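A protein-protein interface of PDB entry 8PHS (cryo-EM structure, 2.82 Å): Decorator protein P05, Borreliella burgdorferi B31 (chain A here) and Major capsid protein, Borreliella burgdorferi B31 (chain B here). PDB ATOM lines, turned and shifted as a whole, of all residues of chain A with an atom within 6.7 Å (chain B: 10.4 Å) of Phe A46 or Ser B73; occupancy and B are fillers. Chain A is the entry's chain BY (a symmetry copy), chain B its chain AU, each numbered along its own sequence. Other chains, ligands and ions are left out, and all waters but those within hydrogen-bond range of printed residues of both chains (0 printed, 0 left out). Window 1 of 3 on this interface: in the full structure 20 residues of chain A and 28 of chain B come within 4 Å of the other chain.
The side-chain amino group (NZ) of Lys A41 lies within salt-bridge range of the side-chain carboxylate (OD1) of Asp B50 (3.1 Å).
The backbone carbonyl oxygen (O) of Asn B54 is in hydrogen-bond range of the side-chain amide nitrogen (ND2) of Asn A42, at 3.3 Å.
The side-chain amino group (NZ) of Lys B48 lies within salt-bridge range of the side-chain carboxylate (OE1) of Glu B75 (3.5 Å).
N of Ser B73 is in hydrogen-bond range of O of Asp B50 (2.9 Å).
The backbone carbonyl oxygen (O) of Phe B52 sits at hydrogen-bond distance from the backbone NH (N) of Gly B71.
The side-chain amide nitrogen (ND2) of Asn B54 sits close to the backbone NH (N) of Gly B71.
The side-chain amide oxygen (OE1) of Gln A26 sits close to the side-chain carboxylate (OE2) of Glu A44 (2.8 Å).
The backbone NH of Phe A46 sits close to the side-chain carboxylate of Glu A44 (3.0 Å).
Among the printed residues, pairs that only touch across the chains: Asn A42 with Leu B53 (3.2 Å), Phe A46 with Phe B52 (3.3 Å), Phe A46 with Ser B73 (3.3 Å), Lys A41 with Phe B52 (3.3 Å), Asn A42 with Phe B52 (3.4 Å), Gln A26 with Glu B75 (3.5 Å), Lys A41 with Ala B51 (3.6 Å) and Phe A46 with Phe B72 (3.96 Å).
Of the 17 printed residues of chain B, 8 touch a printed residue of chain A.
Hydrophobic or aromatic side chains of chain B within 4 Å of the printed part of chain A: Phe B52.
Of the 18 printed residues of chain A, 4 touch a printed residue of chain B.
Among the printed residues, 10 pairs touch across the chains.
Among the printed residues, Asp or Glu carboxylates within 4 Å of a Lys or Arg side-chain nitrogen of the other chain: Lys A41 with Asp B50 (3.1 Å).
Pro A25 touches none of the printed residues of chain B.
Of the printed residues of chain B, Gln A26 touches Glu B75.
Val A43 touches none of the printed residues of chain B.
No residue of chain B comes within 4 Å of Glu A44.
Of chain B, only Phe B52 (3.3 Å), Phe B72 (3.96 Å) and Ser B73 (3.3 Å) come within 4 Å of Phe A46.
No residue of chain B comes within 4 Å of Ala A47.
No residue of chain B comes within 4 Å of Ser A48.
Printed residues of chain A within 4 Å of Ala B51: Lys A41 (3.6 Å).
Printed residues of chain A within 4 Å of Asn B54: Asn A42 (3.3 Å).
Ser B73 touches just one residue of chain A: Phe A46 (3.3 Å).
The nearest residue of chain A that does not touch Ser B73 is Gln A26 (6.4 Å).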
ATOM      1  N   MET A  22     -17.208   9.007   1.511  1.00  0.00           N
ATOM      2  CA  MET A  22     -17.975   8.833   2.738  1.00  0.00           C
ATOM      3  C   MET A  22     -19.100   9.856   2.831  1.00  0.00           C
ATOM      4  O   MET A  22     -19.791  10.123   1.849  1.00  0.00           O
ATOM      5  CB  MET A  22     -17.064   8.942   3.961  1.00  0.00           C
ATOM      6  CG  MET A  22     -16.475   7.619   4.430  1.00  0.00           C
ATOM      7  SD  MET A  22     -17.725   6.367   4.782  1.00  0.00           S
ATOM      8  CE  MET A  22     -17.607   5.338   3.320  1.00  0.00           C
ATOM      9  N   LYS A  23     -19.283  10.420   4.027  1.00  0.00           N
ATOM     10  CA  LYS A  23     -20.302  11.449   4.211  1.00  0.00           C
ATOM     11  C   LYS A  23     -20.000  12.679   3.366  1.00  0.00           C
ATOM     12  O   LYS A  23     -20.902  13.253   2.745  1.00  0.00           O
ATOM     13  CB  LYS A  23     -20.407  11.826   5.688  1.00  0.00           C
ATOM     14  CG  LYS A  23     -21.357  12.978   5.960  1.00  0.00           C
ATOM     15  CD  LYS A  23     -21.188  13.513   7.371  1.00  0.00           C
ATOM     16  CE  LYS A  23     -21.814  14.889   7.510  1.00  0.00           C
ATOM     17  NZ  LYS A  23     -21.660  15.431   8.887  1.00  0.00           N
ATOM     18  N   ASN A  24     -18.734  13.095   3.323  1.00  0.00           N
ATOM     19  CA  ASN A  24     -18.302  14.266   2.560  1.00  0.00           C
ATOM     20  C   ASN A  24     -17.339  13.813   1.473  1.00  0.00           C
ATOM     21  O   ASN A  24     -16.123  13.732   1.701  1.00  0.00           O
ATOM     22  CB  ASN A  24     -17.648  15.305   3.467  1.00  0.00           C
ATOM     23  CG  ASN A  24     -18.605  15.869   4.496  1.00  0.00           C
ATOM     24  OD1 ASN A  24     -19.787  15.530   4.514  1.00  0.00           O
ATOM     25  ND2 ASN A  24     -18.094  16.732   5.366  1.00  0.00           N
ATOM     26  N   PRO A  25     -17.834  13.510   0.274  1.00  0.00           N
ATOM     27  CA  PRO A  25     -16.951  13.145  -0.838  1.00  0.00           C
ATOM     28  C   PRO A  25     -16.390  14.328  -1.609  1.00  0.00           C
ATOM     29  O   PRO A  25     -15.638  14.118  -2.567  1.00  0.00           O
ATOM     30  CB  PRO A  25     -17.884  12.314  -1.725  1.00  0.00           C
ATOM     31  CG  PRO A  25     -19.212  12.978  -1.554  1.00  0.00           C
ATOM     32  CD  PRO A  25     -19.252  13.515  -0.134  1.00  0.00           C
ATOM     33  N   GLN A  26     -16.732  15.555  -1.214  1.00  0.00           N
ATOM     34  CA  GLN A  26     -16.232  16.746  -1.887  1.00  0.00           C
ATOM     35  C   GLN A  26     -14.817  17.117  -1.466  1.00  0.00           C
ATOM     36  O   GLN A  26     -14.244  18.047  -2.039  1.00  0.00           O
ATOM     37  CB  GLN A  26     -17.173  17.925  -1.628  1.00  0.00           C
ATOM     38  CG  GLN A  26     -18.618  17.639  -1.992  1.00  0.00           C
ATOM     39  CD  GLN A  26     -18.773  17.172  -3.424  1.00  0.00           C
ATOM     40  OE1 GLN A  26     -19.190  16.044  -3.678  1.00  0.00           O
ATOM     41  NE2 GLN A  26     -18.439  18.043  -4.370  1.00  0.00           N
ATOM     42  N   LYS A  41     -28.028  24.375  -5.474  1.00  0.00           N
ATOM     43  CA  LYS A  41     -26.755  24.391  -4.771  1.00  0.00           C
ATOM     44  C   LYS A  41     -26.793  23.555  -3.497  1.00  0.00           C
ATOM     45  O   LYS A  41     -25.817  23.556  -2.740  1.00  0.00           O
ATOM     46  CB  LYS A  41     -26.364  25.838  -4.445  1.00  0.00           C
ATOM     47  CG  LYS A  41     -24.876  26.106  -4.323  1.00  0.00           C
ATOM     48  CD  LYS A  41     -24.634  27.567  -3.980  1.00  0.00           C
ATOM     49  CE  LYS A  41     -23.156  27.881  -3.862  1.00  0.00           C
ATOM     50  NZ  LYS A  41     -22.920  29.284  -3.417  1.00  0.00           N
ATOM     51  N   ASN A  42     -27.887  22.833  -3.246  1.00  0.00           N
ATOM     52  CA  ASN A  42     -28.085  22.129  -1.990  1.00  0.00           C
ATOM     53  C   ASN A  42     -28.245  20.624  -2.131  1.00  0.00           C
ATOM     54  O   ASN A  42     -28.185  19.920  -1.117  1.00  0.00           O
ATOM     55  CB  ASN A  42     -29.318  22.683  -1.261  1.00  0.00           C
ATOM     56  CG  ASN A  42     -30.615  22.335  -1.966  1.00  0.00           C
ATOM     57  OD1 ASN A  42     -30.821  22.696  -3.123  1.00  0.00           O
ATOM     58  ND2 ASN A  42     -31.499  21.633  -1.266  1.00  0.00           N
ATOM     59  N   VAL A  43     -28.445  20.108  -3.341  1.00  0.00           N
ATOM     60  CA  VAL A  43     -28.725  18.686  -3.539  1.00  0.00           C
ATOM     61  C   VAL A  43     -27.378  17.986  -3.688  1.00  0.00           C
ATOM     62  O   VAL A  43     -26.826  17.876  -4.782  1.00  0.00           O
ATOM     63  CB  VAL A  43     -29.639  18.442  -4.735  1.00  0.00           C
ATOM     64  CG1 VAL A  43     -30.167  17.019  -4.710  1.00  0.00           C
ATOM     65  CG2 VAL A  43     -30.787  19.440  -4.737  1.00  0.00           C
ATOM     66  N   GLU A  44     -26.841  17.503  -2.570  1.00  0.00           N
ATOM     67  CA  GLU A  44     -25.605  16.738  -2.610  1.00  0.00           C
ATOM     68  C   GLU A  44     -25.596  15.803  -1.407  1.00  0.00           C
ATOM     69  O   GLU A  44     -26.432  15.906  -0.508  1.00  0.00           O
ATOM     70  CB  GLU A  44     -24.381  17.664  -2.624  1.00  0.00           C
ATOM     71  CG  GLU A  44     -23.195  17.172  -3.468  1.00  0.00           C
ATOM     72  CD  GLU A  44     -22.424  16.018  -2.864  1.00  0.00           C
ATOM     73  OE1 GLU A  44     -22.379  15.900  -1.624  1.00  0.00           O
ATOM     74  OE2 GLU A  44     -21.862  15.216  -3.636  1.00  0.00           O
ATOM     75  N   PHE A  45     -24.633  14.880  -1.405  1.00  0.00           N
ATOM     76  CA  PHE A  45     -24.590  13.826  -0.394  1.00  0.00           C
ATOM     77  C   PHE A  45     -24.287  14.366   0.998  1.00  0.00           C
ATOM     78  O   PHE A  45     -24.803  13.837   1.988  1.00  0.00           O
ATOM     79  CB  PHE A  45     -23.552  12.780  -0.796  1.00  0.00           C
ATOM     80  CG  PHE A  45     -23.718  11.463  -0.099  1.00  0.00           C
ATOM     81  CD1 PHE A  45     -24.798  10.646  -0.382  1.00  0.00           C
ATOM     82  CD2 PHE A  45     -22.779  11.029   0.820  1.00  0.00           C
ATOM     83  CE1 PHE A  45     -24.950   9.431   0.252  1.00  0.00           C
ATOM     84  CE2 PHE A  45     -22.924   9.813   1.455  1.00  0.00           C
ATOM     85  CZ  PHE A  45     -24.012   9.013   1.170  1.00  0.00           C
ATOM     86  N   PHE A  46     -23.462  15.410   1.102  1.00  0.00           N
ATOM     87  CA  PHE A  46     -23.035  15.903   2.407  1.00  0.00           C
ATOM     88  C   PHE A  46     -24.139  16.607   3.186  1.00  0.00           C
ATOM     89  O   PHE A  46     -23.933  16.911   4.366  1.00  0.00           O
ATOM     90  CB  PHE A  46     -21.848  16.858   2.257  1.00  0.00           C
ATOM     91  CG  PHE A  46     -22.169  18.103   1.484  1.00  0.00           C
ATOM     92  CD1 PHE A  46     -22.684  19.219   2.118  1.00  0.00           C
ATOM     93  CD2 PHE A  46     -21.912  18.174   0.129  1.00  0.00           C
ATOM     94  CE1 PHE A  46     -22.984  20.351   1.402  1.00  0.00           C
ATOM     95  CE2 PHE A  46     -22.195  19.316  -0.590  1.00  0.00           C
ATOM     96  CZ  PHE A  46     -22.732  20.407   0.048  1.00  0.00           C
ATOM     97  N   ALA A  47     -25.289  16.881   2.572  1.00  0.00           N
ATOM     98  CA  ALA A  47     -26.327  17.686   3.216  1.00  0.00           C
ATOM     99  C   ALA A  47     -26.992  16.855   4.311  1.00  0.00           C
ATOM    100  O   ALA A  47     -28.050  16.248   4.130  1.00  0.00           O
ATOM    101  CB  ALA A  47     -27.342  18.177   2.192  1.00  0.00           C
ATOM    102  N   SER A  48     -26.353  16.840   5.477  1.00  0.00           N
ATOM    103  CA  SER A  48     -26.837  16.081   6.621  1.00  0.00           C
ATOM    104  C   SER A  48     -27.861  16.892   7.404  1.00  0.00           C
ATOM    105  O   SER A  48     -27.687  18.097   7.618  1.00  0.00           O
ATOM    106  CB  SER A  48     -25.678  15.685   7.538  1.00  0.00           C
ATOM    107  OG  SER A  48     -25.004  16.831   8.028  1.00  0.00           O
ATOM    108  N   GLY A  49     -28.931  16.222   7.831  1.00  0.00           N
ATOM    109  CA  GLY A  49     -30.003  16.852   8.573  1.00  0.00           C
ATOM    110  C   GLY A  49     -31.309  16.800   7.795  1.00  0.00           C
ATOM    111  O   GLY A  49     -31.621  15.797   7.142  1.00  0.00           O
ATOM    112  N   TYR A  69     -25.632   5.851   6.569  1.00  0.00           N
ATOM    113  CA  TYR A  69     -25.906   7.272   6.397  1.00  0.00           C
ATOM    114  C   TYR A  69     -27.040   7.494   5.403  1.00  0.00           C
ATOM    115  O   TYR A  69     -27.057   6.904   4.320  1.00  0.00           O
ATOM    116  CB  TYR A  69     -24.646   7.994   5.926  1.00  0.00           C
ATOM    117  CG  TYR A  69     -24.824   9.477   5.696  1.00  0.00           C
ATOM    118  CD1 TYR A  69     -25.339  10.297   6.687  1.00  0.00           C
ATOM    119  CD2 TYR A  69     -24.461  10.056   4.489  1.00  0.00           C
ATOM    120  CE1 TYR A  69     -25.497  11.656   6.480  1.00  0.00           C
ATOM    121  CE2 TYR A  69     -24.615  11.412   4.272  1.00  0.00           C
ATOM    122  CZ  TYR A  69     -25.133  12.206   5.271  1.00  0.00           C
ATOM    123  OH  TYR A  69     -25.287  13.556   5.055  1.00  0.00           O
ATOM    124  N   LYS A  70     -27.985   8.359   5.782  1.00  0.00           N
ATOM    125  CA  LYS A  70     -29.132   8.709   4.945  1.00  0.00           C
ATOM    126  C   LYS A  70     -29.913   7.470   4.519  1.00  0.00           C
ATOM    127  O   LYS A  70     -30.329   7.335   3.367  1.00  0.00           O
ATOM    128  CB  LYS A  70     -28.695   9.524   3.729  1.00  0.00           C
ATOM    129  CG  LYS A  70     -28.436  10.981   4.046  1.00  0.00           C
ATOM    130  CD  LYS A  70     -28.138  11.772   2.792  1.00  0.00           C
ATOM    131  CE  LYS A  70     -28.141  13.258   3.081  1.00  0.00           C
ATOM    132  NZ  LYS A  70     -27.775  14.059   1.882  1.00  0.00           N
ATOM    133  N   ASP A 105     -27.141  11.665  10.121  1.00  0.00           N
ATOM    134  CA  ASP A 105     -25.777  12.160  10.232  1.00  0.00           C
ATOM    135  C   ASP A 105     -24.908  11.067  10.835  1.00  0.00           C
ATOM    136  O   ASP A 105     -25.397  10.180  11.536  1.00  0.00           O
ATOM    137  CB  ASP A 105     -25.707  13.436  11.077  1.00  0.00           C
ATOM    138  CG  ASP A 105     -24.513  14.297  10.733  1.00  0.00           C
ATOM    139  OD1 ASP A 105     -23.684  13.859   9.911  1.00  0.00           O
ATOM    140  OD2 ASP A 105     -24.404  15.415  11.280  1.00  0.00           O
ATOM    141  N   LEU A 176     -30.475  10.390  -4.719  1.00  0.00           N
ATOM    142  CA  LEU A 176     -31.046  11.095  -3.580  1.00  0.00           C
ATOM    143  C   LEU A 176     -32.408  11.655  -3.963  1.00  0.00           C
ATOM    144  O   LEU A 176     -32.542  12.327  -4.990  1.00  0.00           O
ATOM    145  CB  LEU A 176     -30.127  12.223  -3.109  1.00  0.00           C
ATOM    146  CG  LEU A 176     -28.847  11.799  -2.392  1.00  0.00           C
ATOM    147  CD1 LEU A 176     -28.154  13.008  -1.788  1.00  0.00           C
ATOM    148  CD2 LEU A 176     -29.149  10.757  -1.327  1.00  0.00           C
ATOM    149  N   THR B  46      -5.873  23.284   0.409  1.00  0.00           N
ATOM    150  CA  THR B  46      -6.576  24.491   0.820  1.00  0.00           C
ATOM    151  C   THR B  46      -8.011  24.121   1.169  1.00  0.00           C
ATOM    152  O   THR B  46      -8.538  23.109   0.708  1.00  0.00           O
ATOM    153  CB  THR B  46      -6.563  25.570  -0.272  1.00  0.00           C
ATOM    154  OG1 THR B  46      -6.906  24.985  -1.533  1.00  0.00           O
ATOM    155  CG2 THR B  46      -5.191  26.218  -0.371  1.00  0.00           C
ATOM    156  N   VAL B  47      -8.644  24.950   1.994  1.00  0.00           N
ATOM    157  CA  VAL B  47      -9.997  24.698   2.477  1.00  0.00           C
ATOM    158  C   VAL B  47     -10.890  25.851   2.046  1.00  0.00           C
ATOM    159  O   VAL B  47     -10.536  27.020   2.235  1.00  0.00           O
ATOM    160  CB  VAL B  47     -10.030  24.523   4.007  1.00  0.00           C
ATOM    161  CG1 VAL B  47     -11.462  24.392   4.496  1.00  0.00           C
ATOM    162  CG2 VAL B  47      -9.210  23.313   4.419  1.00  0.00           C
ATOM    163  N   LYS B  48     -12.044  25.523   1.466  1.00  0.00           N
ATOM    164  CA  LYS B  48     -13.023  26.519   1.059  1.00  0.00           C
ATOM    165  C   LYS B  48     -14.364  26.201   1.704  1.00  0.00           C
ATOM    166  O   LYS B  48     -14.733  25.031   1.857  1.00  0.00           O
ATOM    167  CB  LYS B  48     -13.161  26.583  -0.471  1.00  0.00           C
ATOM    168  CG  LYS B  48     -13.803  25.360  -1.104  1.00  0.00           C
ATOM    169  CD  LYS B  48     -13.541  25.302  -2.601  1.00  0.00           C
ATOM    170  CE  LYS B  48     -14.231  24.100  -3.224  1.00  0.00           C
ATOM    171  NZ  LYS B  48     -13.827  23.847  -4.629  1.00  0.00           N
ATOM    172  N   TRP B  49     -15.085  27.252   2.089  1.00  0.00           N
ATOM    173  CA  TRP B  49     -16.361  27.131   2.778  1.00  0.00           C
ATOM    174  C   TRP B  49     -17.468  27.714   1.913  1.00  0.00           C
ATOM    175  O   TRP B  49     -17.274  28.735   1.245  1.00  0.00           O
ATOM    176  CB  TRP B  49     -16.327  27.844   4.133  1.00  0.00           C
ATOM    177  CG  TRP B  49     -15.620  27.074   5.207  1.00  0.00           C
ATOM    178  CD1 TRP B  49     -14.359  27.294   5.676  1.00  0.00           C
ATOM    179  CD2 TRP B  49     -16.133  25.960   5.947  1.00  0.00           C
ATOM    180  NE1 TRP B  49     -14.055  26.388   6.662  1.00  0.00           N
ATOM    181  CE2 TRP B  49     -15.127  25.557   6.848  1.00  0.00           C
ATOM    182  CE3 TRP B  49     -17.344  25.263   5.937  1.00  0.00           C
ATOM    183  CZ2 TRP B  49     -15.297  24.492   7.728  1.00  0.00           C
ATOM    184  CZ3 TRP B  49     -17.510  24.205   6.812  1.00  0.00           C
ATOM    185  CH2 TRP B  49     -16.493  23.831   7.697  1.00  0.00           C
ATOM    186  N   ASP B  50     -18.629  27.066   1.933  1.00  0.00           N
ATOM    187  CA  ASP B  50     -19.746  27.435   1.077  1.00  0.00           C
ATOM    188  C   ASP B  50     -21.046  27.325   1.859  1.00  0.00           C
ATOM    189  O   ASP B  50     -21.135  26.582   2.836  1.00  0.00           O
ATOM    190  CB  ASP B  50     -19.799  26.540  -0.167  1.00  0.00           C
ATOM    191  CG  ASP B  50     -20.724  27.076  -1.234  1.00  0.00           C
ATOM    192  OD1 ASP B  50     -21.225  28.210  -1.081  1.00  0.00           O
ATOM    193  OD2 ASP B  50     -20.951  26.358  -2.231  1.00  0.00           O
ATOM    194  N   ALA B  51     -22.057  28.070   1.414  1.00  0.00           N
ATOM    195  CA  ALA B  51     -23.382  28.038   2.015  1.00  0.00           C
ATOM    196  C   ALA B  51     -24.433  27.876   0.928  1.00  0.00           C
ATOM    197  O   ALA B  51     -24.211  28.233  -0.232  1.00  0.00           O
ATOM    198  CB  ALA B  51     -23.669  29.305   2.823  1.00  0.00           C
ATOM    199  N   PHE B  52     -25.584  27.328   1.313  1.00  0.00           N
ATOM    200  CA  PHE B  52     -26.655  27.080   0.358  1.00  0.00           C
ATOM    201  C   PHE B  52     -27.994  27.062   1.080  1.00  0.00           C
ATOM    202  O   PHE B  52     -28.066  26.878   2.298  1.00  0.00           O
ATOM    203  CB  PHE B  52     -26.440  25.764  -0.392  1.00  0.00           C
ATOM    204  CG  PHE B  52     -26.124  24.606   0.505  1.00  0.00           C
ATOM    205  CD1 PHE B  52     -27.138  23.864   1.084  1.00  0.00           C
ATOM    206  CD2 PHE B  52     -24.813  24.266   0.778  1.00  0.00           C
ATOM    207  CE1 PHE B  52     -26.850  22.799   1.910  1.00  0.00           C
ATOM    208  CE2 PHE B  52     -24.521  23.208   1.606  1.00  0.00           C
ATOM    209  CZ  PHE B  52     -25.540  22.472   2.172  1.00  0.00           C
ATOM    210  N   LEU B  53     -29.059  27.241   0.304  1.00  0.00           N
ATOM    211  CA  LEU B  53     -30.425  27.217   0.810  1.00  0.00           C
ATOM    212  C   LEU B  53     -31.035  25.848   0.543  1.00  0.00           C
ATOM    213  O   LEU B  53     -31.006  25.363  -0.592  1.00  0.00           O
ATOM    214  CB  LEU B  53     -31.271  28.306   0.147  1.00  0.00           C
ATOM    215  CG  LEU B  53     -30.681  29.716   0.070  1.00  0.00           C
ATOM    216  CD1 LEU B  53     -31.653  30.663  -0.613  1.00  0.00           C
ATOM    217  CD2 LEU B  53     -30.321  30.229   1.450  1.00  0.00           C
ATOM    218  N   ASN B  54     -31.592  25.233   1.585  1.00  0.00           N
ATOM    219  CA  ASN B  54     -32.156  23.895   1.467  1.00  0.00           C
ATOM    220  C   ASN B  54     -33.589  23.882   0.957  1.00  0.00           C
ATOM    221  O   ASN B  54     -34.016  22.872   0.387  1.00  0.00           O
ATOM    222  CB  ASN B  54     -32.103  23.174   2.817  1.00  0.00           C
ATOM    223  CG  ASN B  54     -30.735  22.610   3.121  1.00  0.00           C
ATOM    224  OD1 ASN B  54     -30.240  21.736   2.412  1.00  0.00           O
ATOM    225  ND2 ASN B  54     -30.110  23.111   4.179  1.00  0.00           N
ATOM    226  N   ILE B  70     -30.569  26.602   6.361  1.00  0.00           N
ATOM    227  CA  ILE B  70     -29.484  26.977   5.461  1.00  0.00           C
ATOM    228  C   ILE B  70     -28.291  26.093   5.792  1.00  0.00           C
ATOM    229  O   ILE B  70     -27.848  26.044   6.945  1.00  0.00           O
ATOM    230  CB  ILE B  70     -29.118  28.464   5.597  1.00  0.00           C
ATOM    231  CG1 ILE B  70     -30.216  29.346   5.002  1.00  0.00           C
ATOM    232  CG2 ILE B  70     -27.780  28.749   4.937  1.00  0.00           C
ATOM    233  CD1 ILE B  70     -29.949  30.826   5.157  1.00  0.00           C
ATOM    234  N   GLY B  71     -27.772  25.395   4.785  1.00  0.00           N
ATOM    235  CA  GLY B  71     -26.689  24.462   4.984  1.00  0.00           C
ATOM    236  C   GLY B  71     -25.335  25.041   4.625  1.00  0.00           C
ATOM    237  O   GLY B  71     -25.228  26.016   3.887  1.00  0.00           O
ATOM    238  N   PHE B  72     -24.291  24.411   5.159  1.00  0.00           N
ATOM    239  CA  PHE B  72     -22.915  24.808   4.908  1.00  0.00           C
ATOM    240  C   PHE B  72     -22.106  23.598   4.465  1.00  0.00           C
ATOM    241  O   PHE B  72     -22.476  22.448   4.718  1.00  0.00           O
ATOM    242  CB  PHE B  72     -22.265  25.437   6.144  1.00  0.00           C
ATOM    243  CG  PHE B  72     -23.015  26.612   6.697  1.00  0.00           C
ATOM    244  CD1 PHE B  72     -24.014  26.434   7.638  1.00  0.00           C
ATOM    245  CD2 PHE B  72     -22.717  27.897   6.281  1.00  0.00           C
ATOM    246  CE1 PHE B  72     -24.702  27.514   8.148  1.00  0.00           C
ATOM    247  CE2 PHE B  72     -23.402  28.980   6.788  1.00  0.00           C
ATOM    248  CZ  PHE B  72     -24.396  28.788   7.723  1.00  0.00           C
ATOM    249  N   SER B  73     -20.989  23.873   3.796  1.00  0.00           N
ATOM    250  CA  SER B  73     -20.140  22.823   3.257  1.00  0.00           C
ATOM    251  C   SER B  73     -18.685  23.258   3.302  1.00  0.00           C
ATOM    252  O   SER B  73     -18.365  24.434   3.116  1.00  0.00           O
ATOM    253  CB  SER B  73     -20.515  22.473   1.816  1.00  0.00           C
ATOM    254  OG  SER B  73     -20.278  23.564   0.947  1.00  0.00           O
ATOM    255  N   SER B  74     -17.809  22.289   3.539  1.00  0.00           N
ATOM    256  CA  SER B  74     -16.369  22.477   3.461  1.00  0.00           C
ATOM    257  C   SER B  74     -15.813  21.574   2.375  1.00  0.00           C
ATOM    258  O   SER B  74     -16.173  20.396   2.292  1.00  0.00           O
ATOM    259  CB  SER B  74     -15.688  22.155   4.788  1.00  0.00           C
ATOM    260  OG  SER B  74     -15.897  20.800   5.142  1.00  0.00           O
ATOM    261  N   GLU B  75     -14.939  22.125   1.540  1.00  0.00           N
ATOM    262  CA  GLU B  75     -14.278  21.336   0.514  1.00  0.00           C
ATOM    263  C   GLU B  75     -12.780  21.589   0.554  1.00  0.00           C
ATOM    264  O   GLU B  75     -12.332  22.731   0.694  1.00  0.00           O
ATOM    265  CB  GLU B  75     -14.825  21.645  -0.880  1.00  0.00           C
ATOM    266  CG  GLU B  75     -16.325  21.467  -1.020  1.00  0.00           C
ATOM    267  CD  GLU B  75     -16.756  21.300  -2.463  1.00  0.00           C
ATOM    268  OE1 GLU B  75     -15.871  21.257  -3.345  1.00  0.00           O
ATOM    269  OE2 GLU B  75     -17.974  21.206  -2.716  1.00  0.00           O
ATOM    270  N   VAL B  76     -12.014  20.511   0.431  1.00  0.00           N
ATOM    271  CA  VAL B  76     -10.560  20.573   0.418  1.00  0.00           C
ATOM    272  C   VAL B  76     -10.101  20.466  -1.029  1.00  0.00           C
ATOM    273  O   VAL B  76     -10.418  19.491  -1.720  1.00  0.00           O
ATOM    274  CB  VAL B  76      -9.941  19.463   1.279  1.00  0.00           C
ATOM    275  CG1 VAL B  76      -8.433  19.623   1.344  1.00  0.00           C
ATOM    276  CG2 VAL B  76     -10.547  19.477   2.672  1.00  0.00           C
ATOM    277  N   ARG B 308     -14.262  27.383 -10.932  1.00  0.00           N
ATOM    278  CA  ARG B 308     -15.211  26.764 -11.849  1.00  0.00           C
ATOM    279  C   ARG B 308     -15.783  27.784 -12.826  1.00  0.00           C
ATOM    280  O   ARG B 308     -16.069  28.928 -12.460  1.00  0.00           O
ATOM    281  CB  ARG B 308     -16.347  26.094 -11.078  1.00  0.00           C
ATOM    282  CG  ARG B 308     -15.973  24.777 -10.427  1.00  0.00           C
ATOM    283  CD  ARG B 308     -17.205  24.013  -9.976  1.00  0.00           C
ATOM    284  NE  ARG B 308     -16.871  22.674  -9.506  1.00  0.00           N
ATOM    285  CZ  ARG B 308     -17.758  21.790  -9.068  1.00  0.00           C
ATOM    286  NH1 ARG B 308     -19.049  22.071  -9.026  1.00  0.00           N
ATOM    287  NH2 ARG B 308     -17.337  20.595  -8.663  1.00  0.00           N
